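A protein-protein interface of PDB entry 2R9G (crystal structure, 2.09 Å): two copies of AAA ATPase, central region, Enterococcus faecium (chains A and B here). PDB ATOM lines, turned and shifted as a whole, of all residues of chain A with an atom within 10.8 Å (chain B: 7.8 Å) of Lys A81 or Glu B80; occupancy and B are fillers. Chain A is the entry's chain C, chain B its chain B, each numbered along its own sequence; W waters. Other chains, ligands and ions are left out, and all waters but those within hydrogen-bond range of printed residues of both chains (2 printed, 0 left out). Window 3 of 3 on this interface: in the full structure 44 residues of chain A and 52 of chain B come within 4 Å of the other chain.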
ATOM      1  N   LEU A  46      -0.151  -2.152 -30.470  1.00  0.00           N
ATOM      2  CA  LEU A  46       1.290  -2.356 -30.317  1.00  0.00           C
ATOM      3  C   LEU A  46       1.655  -3.831 -30.125  1.00  0.00           C
ATOM      4  O   LEU A  46       2.632  -4.314 -30.712  1.00  0.00           O
ATOM      5  CB  LEU A  46       1.829  -1.516 -29.152  1.00  0.00           C
ATOM      6  CG  LEU A  46       3.347  -1.541 -28.967  1.00  0.00           C
ATOM      7  CD1 LEU A  46       4.014  -0.935 -30.181  1.00  0.00           C
ATOM      8  CD2 LEU A  46       3.762  -0.838 -27.667  1.00  0.00           C
ATOM      9  N   ALA A  47       0.863  -4.538 -29.312  1.00  0.00           N
ATOM     10  CA  ALA A  47       1.082  -5.968 -29.072  1.00  0.00           C
ATOM     11  C   ALA A  47       1.073  -6.783 -30.369  1.00  0.00           C
ATOM     12  O   ALA A  47       1.866  -7.714 -30.508  1.00  0.00           O
ATOM     13  CB  ALA A  47       0.076  -6.517 -28.073  1.00  0.00           C
ATOM     14  N   CYS A  50       4.306  -5.961 -32.518  1.00  0.00           N
ATOM     15  CA  CYS A  50       5.436  -6.629 -31.906  1.00  0.00           C
ATOM     16  C   CYS A  50       5.476  -8.106 -32.264  1.00  0.00           C
ATOM     17  O   CYS A  50       6.543  -8.635 -32.596  1.00  0.00           O
ATOM     18  CB  CYS A  50       5.397  -6.446 -30.391  1.00  0.00           C
ATOM     19  SG  CYS A  50       5.827  -4.794 -29.850  1.00  0.00           S
ATOM     20  N   VAL A  73      13.554  -9.137 -30.751  1.00  0.00           N
ATOM     21  CA  VAL A  73      13.072  -9.451 -29.415  1.00  0.00           C
ATOM     22  C   VAL A  73      13.501  -8.351 -28.432  1.00  0.00           C
ATOM     23  O   VAL A  73      12.696  -7.908 -27.624  1.00  0.00           O
ATOM     24  CB  VAL A  73      13.547 -10.848 -28.975  1.00  0.00           C
ATOM     25  CG1 VAL A  73      13.011 -11.202 -27.592  1.00  0.00           C
ATOM     26  CG2 VAL A  73      13.115 -11.891 -30.014  1.00  0.00           C
ATOM     27  N   ASN A  74      14.746  -7.883 -28.539  1.00  0.00           N
ATOM     28  CA  ASN A  74      15.204  -6.737 -27.747  1.00  0.00           C
ATOM     29  C   ASN A  74      14.299  -5.527 -27.965  1.00  0.00           C
ATOM     30  O   ASN A  74      13.790  -4.951 -27.001  1.00  0.00           O
ATOM     31  CB  ASN A  74      16.671  -6.374 -28.062  1.00  0.00           C
ATOM     32  CG  ASN A  74      17.646  -7.472 -27.673  1.00  0.00           C
ATOM     33  OD1 ASN A  74      17.636  -8.565 -28.248  1.00  0.00           O
ATOM     34  ND2 ASN A  74      18.507  -7.183 -26.700  1.00  0.00           N
ATOM     35  N   ALA A  75      14.066  -5.191 -29.238  1.00  0.00           N
ATOM     36  CA  ALA A  75      13.228  -4.056 -29.633  1.00  0.00           C
ATOM     37  C   ALA A  75      11.796  -4.158 -29.111  1.00  0.00           C
ATOM     38  O   ALA A  75      11.227  -3.160 -28.696  1.00  0.00           O
ATOM     39  CB  ALA A  75      13.231  -3.892 -31.140  1.00  0.00           C
ATOM     40  N   VAL A  76      11.245  -5.370 -29.120  1.00  0.00           N
ATOM     41  CA  VAL A  76       9.896  -5.650 -28.631  1.00  0.00           C
ATOM     42  C   VAL A  76       9.803  -5.450 -27.120  1.00  0.00           C
ATOM     43  O   VAL A  76       8.823  -4.881 -26.629  1.00  0.00           O
ATOM     44  CB  VAL A  76       9.427  -7.069 -29.069  1.00  0.00           C
ATOM     45  CG1 VAL A  76       8.235  -7.586 -28.223  1.00  0.00           C
ATOM     46  CG2 VAL A  76       9.075  -7.058 -30.555  1.00  0.00           C
ATOM     47  N   LEU A  77      10.837  -5.881 -26.396  1.00  0.00           N
ATOM     48  CA  LEU A  77      10.892  -5.690 -24.947  1.00  0.00           C
ATOM     49  C   LEU A  77      11.008  -4.215 -24.613  1.00  0.00           C
ATOM     50  O   LEU A  77      10.440  -3.756 -23.623  1.00  0.00           O
ATOM     51  CB  LEU A  77      12.042  -6.475 -24.304  1.00  0.00           C
ATOM     52  CG  LEU A  77      11.982  -8.008 -24.310  1.00  0.00           C
ATOM     53  CD1 LEU A  77      13.270  -8.591 -23.760  1.00  0.00           C
ATOM     54  CD2 LEU A  77      10.778  -8.541 -23.543  1.00  0.00           C
ATOM     55  N   ALA A  78      11.729  -3.480 -25.457  1.00  0.00           N
ATOM     56  CA  ALA A  78      11.813  -2.023 -25.358  1.00  0.00           C
ATOM     57  C   ALA A  78      10.436  -1.371 -25.594  1.00  0.00           C
ATOM     58  O   ALA A  78      10.037  -0.492 -24.844  1.00  0.00           O
ATOM     59  CB  ALA A  78      12.860  -1.476 -26.352  1.00  0.00           C
ATOM     60  N   ALA A  79       9.720  -1.838 -26.621  1.00  0.00           N
ATOM     61  CA  ALA A  79       8.365  -1.368 -26.972  1.00  0.00           C
ATOM     62  C   ALA A  79       7.306  -1.571 -25.883  1.00  0.00           C
ATOM     63  O   ALA A  79       6.528  -0.655 -25.603  1.00  0.00           O
ATOM     64  CB  ALA A  79       7.905  -2.021 -28.283  1.00  0.00           C
ATOM     65  N   GLU A  80       7.281  -2.762 -25.284  1.00  0.00           N
ATOM     66  CA  GLU A  80       6.410  -3.066 -24.132  1.00  0.00           C
ATOM     67  C   GLU A  80       6.673  -2.150 -22.938  1.00  0.00           C
ATOM     68  O   GLU A  80       5.737  -1.696 -22.271  1.00  0.00           O
ATOM     69  CB  GLU A  80       6.613  -4.513 -23.668  1.00  0.00           C
ATOM     70  CG  GLU A  80       6.140  -5.567 -24.632  1.00  0.00           C
ATOM     71  CD  GLU A  80       6.742  -6.933 -24.343  1.00  0.00           C
ATOM     72  OE1 GLU A  80       7.376  -7.107 -23.277  1.00  0.00           O
ATOM     73  OE2 GLU A  80       6.582  -7.835 -25.190  1.00  0.00           O
ATOM     74  N   LYS A  81       7.949  -1.889 -22.663  1.00  0.00           N
ATOM     75  CA  LYS A  81       8.332  -1.020 -21.547  1.00  0.00           C
ATOM     76  C   LYS A  81       7.992   0.444 -21.809  1.00  0.00           C
ATOM     77  O   LYS A  81       7.648   1.168 -20.879  1.00  0.00           O
ATOM     78  CB  LYS A  81       9.817  -1.167 -21.217  1.00  0.00           C
ATOM     79  CG  LYS A  81      10.164  -2.492 -20.555  1.00  0.00           C
ATOM     80  CD  LYS A  81      11.672  -2.759 -20.580  1.00  0.00           C
ATOM     81  CE  LYS A  81      11.979  -4.192 -20.168  1.00  0.00           C
ATOM     82  NZ  LYS A  81      11.514  -4.495 -18.787  1.00  0.00           N
ATOM     83  N   LEU A  82       8.062   0.859 -23.076  1.00  0.00           N
ATOM     84  CA  LEU A  82       7.864   2.257 -23.459  1.00  0.00           C
ATOM     85  C   LEU A  82       6.412   2.606 -23.751  1.00  0.00           C
ATOM     86  O   LEU A  82       5.936   3.675 -23.357  1.00  0.00           O
ATOM     87  CB  LEU A  82       8.718   2.619 -24.690  1.00  0.00           C
ATOM     88  CG  LEU A  82      10.241   2.634 -24.518  1.00  0.00           C
ATOM     89  CD1 LEU A  82      10.955   2.778 -25.876  1.00  0.00           C
ATOM     90  CD2 LEU A  82      10.699   3.682 -23.532  1.00  0.00           C
ATOM     91  N   GLY A  83       5.729   1.713 -24.472  1.00  0.00           N
ATOM     92  CA  GLY A  83       4.421   1.991 -25.047  1.00  0.00           C
ATOM     93  C   GLY A  83       4.536   3.002 -26.178  1.00  0.00           C
ATOM     94  O   GLY A  83       5.580   3.629 -26.368  1.00  0.00           O
ATOM     95  N   LEU A  84       3.467   3.147 -26.947  1.00  0.00           N
ATOM     96  CA  LEU A  84       3.374   4.215 -27.933  1.00  0.00           C
ATOM     97  C   LEU A  84       3.159   5.541 -27.199  1.00  0.00           C
ATOM     98  O   LEU A  84       2.503   5.556 -26.150  1.00  0.00           O
ATOM     99  CB  LEU A  84       2.224   3.930 -28.903  1.00  0.00           C
ATOM    100  CG  LEU A  84       2.463   2.733 -29.819  1.00  0.00           C
ATOM    101  CD1 LEU A  84       1.169   2.356 -30.493  1.00  0.00           C
ATOM    102  CD2 LEU A  84       3.571   3.030 -30.844  1.00  0.00           C
ATOM    103  N   PRO A  85       3.677   6.660 -27.742  1.00  0.00           N
ATOM    104  CA  PRO A  85       4.316   6.867 -29.047  1.00  0.00           C
ATOM    105  C   PRO A  85       5.773   6.412 -29.176  1.00  0.00           C
ATOM    106  O   PRO A  85       6.205   6.106 -30.281  1.00  0.00           O
ATOM    107  CB  PRO A  85       4.229   8.383 -29.239  1.00  0.00           C
ATOM    108  CG  PRO A  85       4.306   8.930 -27.845  1.00  0.00           C
ATOM    109  CD  PRO A  85       3.604   7.917 -26.966  1.00  0.00           C
ATOM    110  N   GLU A  86       6.514   6.354 -28.070  1.00  0.00           N
ATOM    111  CA  GLU A  86       7.961   6.108 -28.123  1.00  0.00           C
ATOM    112  C   GLU A  86       8.360   4.717 -28.611  1.00  0.00           C
ATOM    113  O   GLU A  86       9.442   4.557 -29.176  1.00  0.00           O
ATOM    114  CB  GLU A  86       8.616   6.405 -26.774  1.00  0.00           C
ATOM    115  CG  GLU A  86       8.775   7.892 -26.504  1.00  0.00           C
ATOM    116  CD  GLU A  86       9.388   8.190 -25.149  1.00  0.00           C
ATOM    117  OE1 GLU A  86       8.981   7.562 -24.147  1.00  0.00           O
ATOM    118  OE2 GLU A  86      10.282   9.062 -25.089  1.00  0.00           O
ATOM    119  N   ALA A  87       7.480   3.731 -28.412  1.00  0.00           N
ATOM    120  CA  ALA A  87       7.690   2.356 -28.891  1.00  0.00           C
ATOM    121  C   ALA A  87       8.000   2.264 -30.380  1.00  0.00           C
ATOM    122  O   ALA A  87       8.689   1.342 -30.808  1.00  0.00           O
ATOM    123  CB  ALA A  87       6.488   1.508 -28.588  1.00  0.00           C
ATOM    124  N   ARG A  88       7.487   3.225 -31.152  1.00  0.00           N
ATOM    125  CA  ARG A  88       7.655   3.264 -32.606  1.00  0.00           C
ATOM    126  C   ARG A  88       9.119   3.371 -33.045  1.00  0.00           C
ATOM    127  O   ARG A  88       9.458   3.014 -34.180  1.00  0.00           O
ATOM    128  CB  ARG A  88       6.848   4.432 -33.197  1.00  0.00           C
ATOM    129  CG  ARG A  88       7.609   5.769 -33.278  1.00  0.00           C
ATOM    130  CD  ARG A  88       6.686   6.963 -33.482  1.00  0.00           C
ATOM    131  NE  ARG A  88       7.433   8.223 -33.560  1.00  0.00           N
ATOM    132  CZ  ARG A  88       7.863   8.924 -32.509  1.00  0.00           C
ATOM    133  NH1 ARG A  88       8.527  10.054 -32.702  1.00  0.00           N
ATOM    134  NH2 ARG A  88       7.644   8.505 -31.267  1.00  0.00           N
ATOM    135  N   PRO A  90      12.289   2.003 -31.522  1.00  0.00           N
ATOM    136  CA  PRO A  90      12.934   0.701 -31.763  1.00  0.00           C
ATOM    137  C   PRO A  90      12.347  -0.139 -32.908  1.00  0.00           C
ATOM    138  O   PRO A  90      13.098  -0.824 -33.606  1.00  0.00           O
ATOM    139  CB  PRO A  90      12.770  -0.042 -30.420  1.00  0.00           C
ATOM    140  CG  PRO A  90      11.780   0.735 -29.636  1.00  0.00           C
ATOM    141  CD  PRO A  90      11.898   2.143 -30.104  1.00  0.00           C
ATOM    142  N   LEU A  91      11.032  -0.077 -33.103  1.00  0.00           N
ATOM    143  CA  LEU A  91      10.381  -0.826 -34.189  1.00  0.00           C
ATOM    144  C   LEU A  91      10.823  -0.355 -35.563  1.00  0.00           C
ATOM    145  O   LEU A  91      11.027  -1.177 -36.448  1.00  0.00           O
ATOM    146  CB  LEU A  91       8.860  -0.751 -34.090  1.00  0.00           C
ATOM    147  CG  LEU A  91       8.279  -1.332 -32.802  1.00  0.00           C
ATOM    148  CD1 LEU A  91       6.782  -1.173 -32.803  1.00  0.00           C
ATOM    149  CD2 LEU A  91       8.703  -2.805 -32.612  1.00  0.00           C
ATOM    150  N   LEU B  46      14.547   4.934 -11.185  1.00  0.00           N
ATOM    151  CA  LEU B  46      15.295   4.040 -12.067  1.00  0.00           C
ATOM    152  C   LEU B  46      14.559   3.678 -13.364  1.00  0.00           C
ATOM    153  O   LEU B  46      15.177   3.631 -14.437  1.00  0.00           O
ATOM    154  CB  LEU B  46      15.720   2.773 -11.315  1.00  0.00           C
ATOM    155  CG  LEU B  46      16.467   1.674 -12.082  1.00  0.00           C
ATOM    156  CD1 LEU B  46      17.845   2.154 -12.512  1.00  0.00           C
ATOM    157  CD2 LEU B  46      16.551   0.384 -11.266  1.00  0.00           C
ATOM    158  N   ALA B  47      13.247   3.449 -13.271  1.00  0.00           N
ATOM    159  CA  ALA B  47      12.460   3.038 -14.438  1.00  0.00           C
ATOM    160  C   ALA B  47      12.421   4.146 -15.469  1.00  0.00           C
ATOM    161  O   ALA B  47      12.443   3.880 -16.665  1.00  0.00           O
ATOM    162  CB  ALA B  47      11.060   2.633 -14.040  1.00  0.00           C
ATOM    163  N   CYS B  50      15.836   4.204 -17.270  1.00  0.00           N
ATOM    164  CA  CYS B  50      15.843   3.061 -18.183  1.00  0.00           C
ATOM    165  C   CYS B  50      15.042   3.283 -19.462  1.00  0.00           C
ATOM    166  O   CYS B  50      15.513   2.947 -20.553  1.00  0.00           O
ATOM    167  CB  CYS B  50      15.340   1.827 -17.450  1.00  0.00           C
ATOM    168  SG  CYS B  50      16.512   1.229 -16.241  1.00  0.00           S
ATOM    169  N   ARG B  51      13.860   3.882 -19.316  1.00  0.00           N
ATOM    170  CA  ARG B  51      13.027   4.295 -20.450  1.00  0.00           C
ATOM    171  C   ARG B  51      13.726   5.288 -21.371  1.00  0.00           C
ATOM    172  O   ARG B  51      13.690   5.132 -22.595  1.00  0.00           O
ATOM    173  CB  ARG B  51      11.697   4.884 -19.961  1.00  0.00           C
ATOM    174  CG  ARG B  51      10.593   3.859 -19.764  1.00  0.00           C
ATOM    175  CD  ARG B  51       9.298   4.513 -19.255  1.00  0.00           C
ATOM    176  NE  ARG B  51       9.037   4.169 -17.855  1.00  0.00           N
ATOM    177  CZ  ARG B  51       8.868   5.046 -16.871  1.00  0.00           C
ATOM    178  NH1 ARG B  51       8.920   6.341 -17.112  1.00  0.00           N
ATOM    179  NH2 ARG B  51       8.633   4.625 -15.639  1.00  0.00           N
ATOM    180  N   ARG B  52      14.369   6.294 -20.780  1.00  0.00           N
ATOM    181  CA  ARG B  52      15.101   7.313 -21.530  1.00  0.00           C
ATOM    182  C   ARG B  52      16.278   6.733 -22.301  1.00  0.00           C
ATOM    183  O   ARG B  52      16.488   7.060 -23.460  1.00  0.00           O
ATOM    184  CB  ARG B  52      15.597   8.423 -20.596  1.00  0.00           C
ATOM    185  CG  ARG B  52      14.516   9.174 -19.828  1.00  0.00           C
ATOM    186  CD  ARG B  52      13.458   9.792 -20.724  1.00  0.00           C
ATOM    187  NE  ARG B  52      12.268   8.953 -20.825  1.00  0.00           N
ATOM    188  CZ  ARG B  52      11.592   8.747 -21.947  1.00  0.00           C
ATOM    189  NH1 ARG B  52      11.997   9.305 -23.082  1.00  0.00           N
ATOM    190  NH2 ARG B  52      10.519   7.967 -21.936  1.00  0.00           N
ATOM    191  N   MET B  54      16.788   3.567 -23.330  1.00  0.00           N
ATOM    192  CA  MET B  54      16.321   2.728 -24.445  1.00  0.00           C
ATOM    193  C   MET B  54      15.895   3.623 -25.615  1.00  0.00           C
ATOM    194  O   MET B  54      16.283   3.373 -26.763  1.00  0.00           O
ATOM    195  CB  MET B  54      15.197   1.756 -24.015  1.00  0.00           C
ATOM    196  CG  MET B  54      15.679   0.377 -23.418  1.00  0.00           C
ATOM    197  SD  MET B  54      14.335  -0.678 -22.694  1.00  0.00           S
ATOM    198  CE  MET B  54      13.452   0.541 -21.798  1.00  0.00           C
ATOM    199  N   VAL B  73      18.764  -2.701 -23.812  1.00  0.00           N
ATOM    200  CA  VAL B  73      17.652  -3.481 -23.292  1.00  0.00           C
ATOM    201  C   VAL B  73      18.176  -4.528 -22.305  1.00  0.00           C
ATOM    202  O   VAL B  73      17.623  -4.682 -21.215  1.00  0.00           O
ATOM    203  CB  VAL B  73      16.855  -4.148 -24.438  1.00  0.00           C
ATOM    204  CG1 VAL B  73      15.665  -4.899 -23.890  1.00  0.00           C
ATOM    205  CG2 VAL B  73      16.403  -3.096 -25.468  1.00  0.00           C
ATOM    206  N   ASN B  74      19.258  -5.214 -22.674  1.00  0.00           N
ATOM    207  CA  ASN B  74      19.952  -6.119 -21.747  1.00  0.00           C
ATOM    208  C   ASN B  74      20.350  -5.435 -20.438  1.00  0.00           C
ATOM    209  O   ASN B  74      20.145  -6.005 -19.376  1.00  0.00           O
ATOM    210  CB  ASN B  74      21.179  -6.780 -22.394  1.00  0.00           C
ATOM    211  CG  ASN B  74      20.816  -7.650 -23.587  1.00  0.00           C
ATOM    212  OD1 ASN B  74      20.272  -7.160 -24.572  1.00  0.00           O
ATOM    213  ND2 ASN B  74      21.134  -8.940 -23.510  1.00  0.00           N
ATOM    214  N   ALA B  75      20.903  -4.217 -20.530  1.00  0.00           N
ATOM    215  CA  ALA B  75      21.337  -3.449 -19.349  1.00  0.00           C
ATOM    216  C   ALA B  75      20.174  -2.988 -18.471  1.00  0.00           C
ATOM    217  O   ALA B  75      20.278  -3.000 -17.247  1.00  0.00           O
ATOM    218  CB  ALA B  75      22.182  -2.251 -19.762  1.00  0.00           C
ATOM    219  N   VAL B  76      19.085  -2.579 -19.114  1.00  0.00           N
ATOM    220  CA  VAL B  76      17.837  -2.202 -18.441  1.00  0.00           C
ATOM    221  C   VAL B  76      17.250  -3.384 -17.664  1.00  0.00           C
ATOM    222  O   VAL B  76      16.853  -3.228 -16.505  1.00  0.00           O
ATOM    223  CB  VAL B  76      16.810  -1.606 -19.452  1.00  0.00           C
ATOM    224  CG1 VAL B  76      15.379  -1.622 -18.895  1.00  0.00           C
ATOM    225  CG2 VAL B  76      17.215  -0.202 -19.842  1.00  0.00           C
ATOM    226  N   LEU B  77      17.231  -4.563 -18.291  1.00  0.00           N
ATOM    227  CA  LEU B  77      16.795  -5.793 -17.623  1.00  0.00           C
ATOM    228  C   LEU B  77      17.659  -6.121 -16.398  1.00  0.00           C
ATOM    229  O   LEU B  77      17.128  -6.501 -15.358  1.00  0.00           O
ATOM    230  CB  LEU B  77      16.765  -6.979 -18.597  1.00  0.00           C
ATOM    231  CG  LEU B  77      15.703  -7.009 -19.703  1.00  0.00           C
ATOM    232  CD1 LEU B  77      15.934  -8.202 -20.625  1.00  0.00           C
ATOM    233  CD2 LEU B  77      14.286  -7.029 -19.126  1.00  0.00           C
ATOM    234  N   ALA B  78      18.976  -5.952 -16.532  1.00  0.00           N
ATOM    235  CA  ALA B  78      19.911  -6.096 -15.420  1.00  0.00           C
ATOM    236  C   ALA B  78      19.605  -5.065 -14.331  1.00  0.00           C
ATOM    237  O   ALA B  78      19.461  -5.415 -13.151  1.00  0.00           O
ATOM    238  CB  ALA B  78      21.347  -5.960 -15.905  1.00  0.00           C
ATOM    239  N   ALA B  79      19.457  -3.809 -14.745  1.00  0.00           N
ATOM    240  CA  ALA B  79      19.109  -2.711 -13.836  1.00  0.00           C
ATOM    241  C   ALA B  79      17.864  -2.981 -13.011  1.00  0.00           C
ATOM    242  O   ALA B  79      17.869  -2.742 -11.802  1.00  0.00           O
ATOM    243  CB  ALA B  79      18.957  -1.402 -14.595  1.00  0.00           C
ATOM    244  N   GLU B  80      16.807  -3.468 -13.671  1.00  0.00           N
ATOM    245  CA  GLU B  80      15.543  -3.812 -13.007  1.00  0.00           C
ATOM    246  C   GLU B  80      15.739  -4.920 -11.980  1.00  0.00           C
ATOM    247  O   GLU B  80      15.232  -4.830 -10.874  1.00  0.00           O
ATOM    248  CB  GLU B  80      14.485  -4.277 -14.020  1.00  0.00           C
ATOM    249  CG  GLU B  80      13.905  -3.202 -14.916  1.00  0.00           C
ATOM    250  CD  GLU B  80      13.022  -3.781 -16.012  1.00  0.00           C
ATOM    251  OE1 GLU B  80      13.048  -5.013 -16.224  1.00  0.00           O
ATOM    252  OE2 GLU B  80      12.295  -3.009 -16.672  1.00  0.00           O
ATOM    253  N   LYS B  81      16.478  -5.963 -12.355  1.00  0.00           N
ATOM    254  CA  LYS B  81      16.727  -7.099 -11.464  1.00  0.00           C
ATOM    255  C   LYS B  81      17.640  -6.754 -10.278  1.00  0.00           C
ATOM    256  O   LYS B  81      17.491  -7.315  -9.187  1.00  0.00           O
ATOM    257  CB  LYS B  81      17.277  -8.279 -12.253  1.00  0.00           C
ATOM    258  CG  LYS B  81      16.258  -8.899 -13.190  1.00  0.00           C
ATOM    259  CD  LYS B  81      16.924  -9.843 -14.169  1.00  0.00           C
ATOM    260  CE  LYS B  81      15.904 -10.510 -15.058  1.00  0.00           C
ATOM    261  NZ  LYS B  81      14.993 -11.426 -14.302  1.00  0.00           N
ATOM    262  N   LEU B  82      18.562  -5.820 -10.493  1.00  0.00           N
ATOM    263  CA  LEU B  82      19.488  -5.380  -9.448  1.00  0.00           C
ATOM    264  C   LEU B  82      18.908  -4.293  -8.544  1.00  0.00           C
ATOM    265  O   LEU B  82      19.020  -4.370  -7.320  1.00  0.00           O
ATOM    266  CB  LEU B  82      20.802  -4.869 -10.069  1.00  0.00           C
ATOM    267  CG  LEU B  82      21.642  -5.874 -10.861  1.00  0.00           C
ATOM    268  CD1 LEU B  82      22.794  -5.169 -11.569  1.00  0.00           C
ATOM    269  CD2 LEU B  82      22.136  -7.020  -9.989  1.00  0.00           C
ATOM    270  N   GLY B  83      18.322  -3.266  -9.157  1.00  0.00           N
ATOM    271  CA  GLY B  83      17.930  -2.060  -8.447  1.00  0.00           C
ATOM    272  C   GLY B  83      19.132  -1.204  -8.065  1.00  0.00           C
ATOM    273  O   GLY B  83      20.286  -1.660  -8.116  1.00  0.00           O
ATOM    274  N   LEU B  84      18.862   0.046  -7.696  1.00  0.00           N
ATOM    275  CA  LEU B  84      19.904   0.967  -7.245  1.00  0.00           C
ATOM    276  C   LEU B  84      20.390   0.528  -5.856  1.00  0.00           C
ATOM    277  O   LEU B  84      19.601   0.007  -5.077  1.00  0.00           O
ATOM    278  CB  LEU B  84      19.379   2.415  -7.233  1.00  0.00           C
ATOM    279  CG  LEU B  84      19.121   3.102  -8.586  1.00  0.00           C
ATOM    280  CD1 LEU B  84      18.324   4.375  -8.392  1.00  0.00           C
ATOM    281  CD2 LEU B  84      20.411   3.391  -9.387  1.00  0.00           C
ATOM    282  N   ALA B  87      22.364  -0.993 -10.012  1.00  0.00           N
ATOM    283  CA  ALA B  87      21.775  -0.727 -11.330  1.00  0.00           C
ATOM    284  C   ALA B  87      22.515   0.345 -12.117  1.00  0.00           C
ATOM    285  O   ALA B  87      22.468   0.348 -13.350  1.00  0.00           O
ATOM    286  CB  ALA B  87      20.317  -0.331 -11.187  1.00  0.00           C
ATOM    287  N   PRO B  90      25.418  -1.235 -14.978  1.00  0.00           N
ATOM    288  CA  PRO B  90      25.107  -1.447 -16.398  1.00  0.00           C
ATOM    289  C   PRO B  90      24.726  -0.173 -17.160  1.00  0.00           C
ATOM    290  O   PRO B  90      25.051  -0.059 -18.335  1.00  0.00           O
ATOM    291  CB  PRO B  90      23.922  -2.434 -16.374  1.00  0.00           C
ATOM    292  CG  PRO B  90      23.403  -2.422 -14.986  1.00  0.00           C
ATOM    293  CD  PRO B  90      24.568  -2.080 -14.109  1.00  0.00           C
ATOM    294  N   LEU B  91      24.052   0.761 -16.494  1.00  0.00           N
ATOM    295  CA  LEU B  91      23.642   2.008 -17.135  1.00  0.00           C
ATOM    296  C   LEU B  91      24.837   2.848 -17.561  1.00  0.00           C
ATOM    297  O   LEU B  91      24.866   3.350 -18.682  1.00  0.00           O
ATOM    298  CB  LEU B  91      22.684   2.802 -16.248  1.00  0.00           C
ATOM    299  CG  LEU B  91      21.362   2.105 -15.879  1.00  0.00           C
ATOM    300  CD1 LEU B  91      20.561   2.976 -14.958  1.00  0.00           C
ATOM    301  CD2 LEU B  91      20.530   1.698 -17.078  1.00  0.00           C
HETATM  302  O   HOH W   1       9.251   1.027 -18.108  1.00  0.00           O
HETATM  303  O   HOH W   2      21.419  -7.902 -26.786  1.00  0.00           O
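Asn A74 touches Val B73, but with the chains exchanged Val A73 does not touch Asn B74 (7.9 Å). Asn A74 touches its own counterpart, Asn B74. Ala A78 touches Val B73, but with the chains exchanged Val A73 does not touch Ala B78 (12.9 Å). Lys A81 touches Glu B80, but with the chains exchanged Glu A80 does not touch Lys B81 (12.3 Å). 18 positions are printed for both chains.
Of chain A, only Lys A81 comes within 4 Å of Glu B80. No residue of chain A comes within 4 Å of Val B76. No residue of chain A comes within 4 Å of Ala B78. No residue of chain A comes within 4 Å of Ala B79. Gly B83 touches none of the printed residues of chain A. Printed residues of chain A within 4 Å of Arg B52: Glu A86 (2.7 Å). Of the printed residues of chain B, Leu A77 touches Val B73 (3.97 Å). Printed residues of chain A within 4 Å of Val B73: Asn A74, Leu A77 and Ala A78. Printed residues of chain B within 4 Å of Asn A74: Val B73 (3.6 Å) and Asn B74 (2.8 Å). Ala A75 touches none of the printed residues of chain B. Leu B91 touches none of the printed residues of chain A. The nearest printed residue of chain B that does not touch Asn A74 is Met B54 (6.1 Å).
Water W2 bridges OD1 of Asn B74 and ND2 of Asn A74. Water W1 lies within hydrogen-bond range of NE of Arg B51 and O of Lys A81.
Asn A74 touches Val B73. Val B73 touches Leu A77. Met B54 touches Ala A78 (SD to CA, 3.9 Å). Ala A78 touches Val B73 (CB to CG2, 3.99 Å). Lys A81 touches Met B54. NZ of Lys A81 touches CD2 of Leu B77, 3.8 Å away. Arg B51 touches Leu A82 (O to CD2, 3.5 Å).
The side-chain carboxylate (OE2) of Glu A86 is in salt-bridge range of the guanidinium group (NH1) of Arg B52 (2.7 Å). ND2 of Asn A74 lies within hydrogen-bond range of OD1 of Asn B74, at 2.8 Å. The side-chain carboxylate (OE2) of Glu B80 is in salt-bridge range of the side-chain amino group (NZ) of Lys A81 (2.7 Å).
Printed residues of chain A that touch a printed residue of chain B: Asn A74, Leu A77, Ala A78, Lys A81, Leu A82 and Glu A86. Of the 21 printed residues of chain B, 7 touch a printed residue of chain A. Printed residues of chain B that touch a printed residue of chain A: Arg B51, Arg B52, Met B54, Val B73, Asn B74, Leu B77 and Glu B80. Hydrophobic or aromatic side chains of chain B within 4 Å of the printed part of chain A: Met B54, Val B73 and Leu B77.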
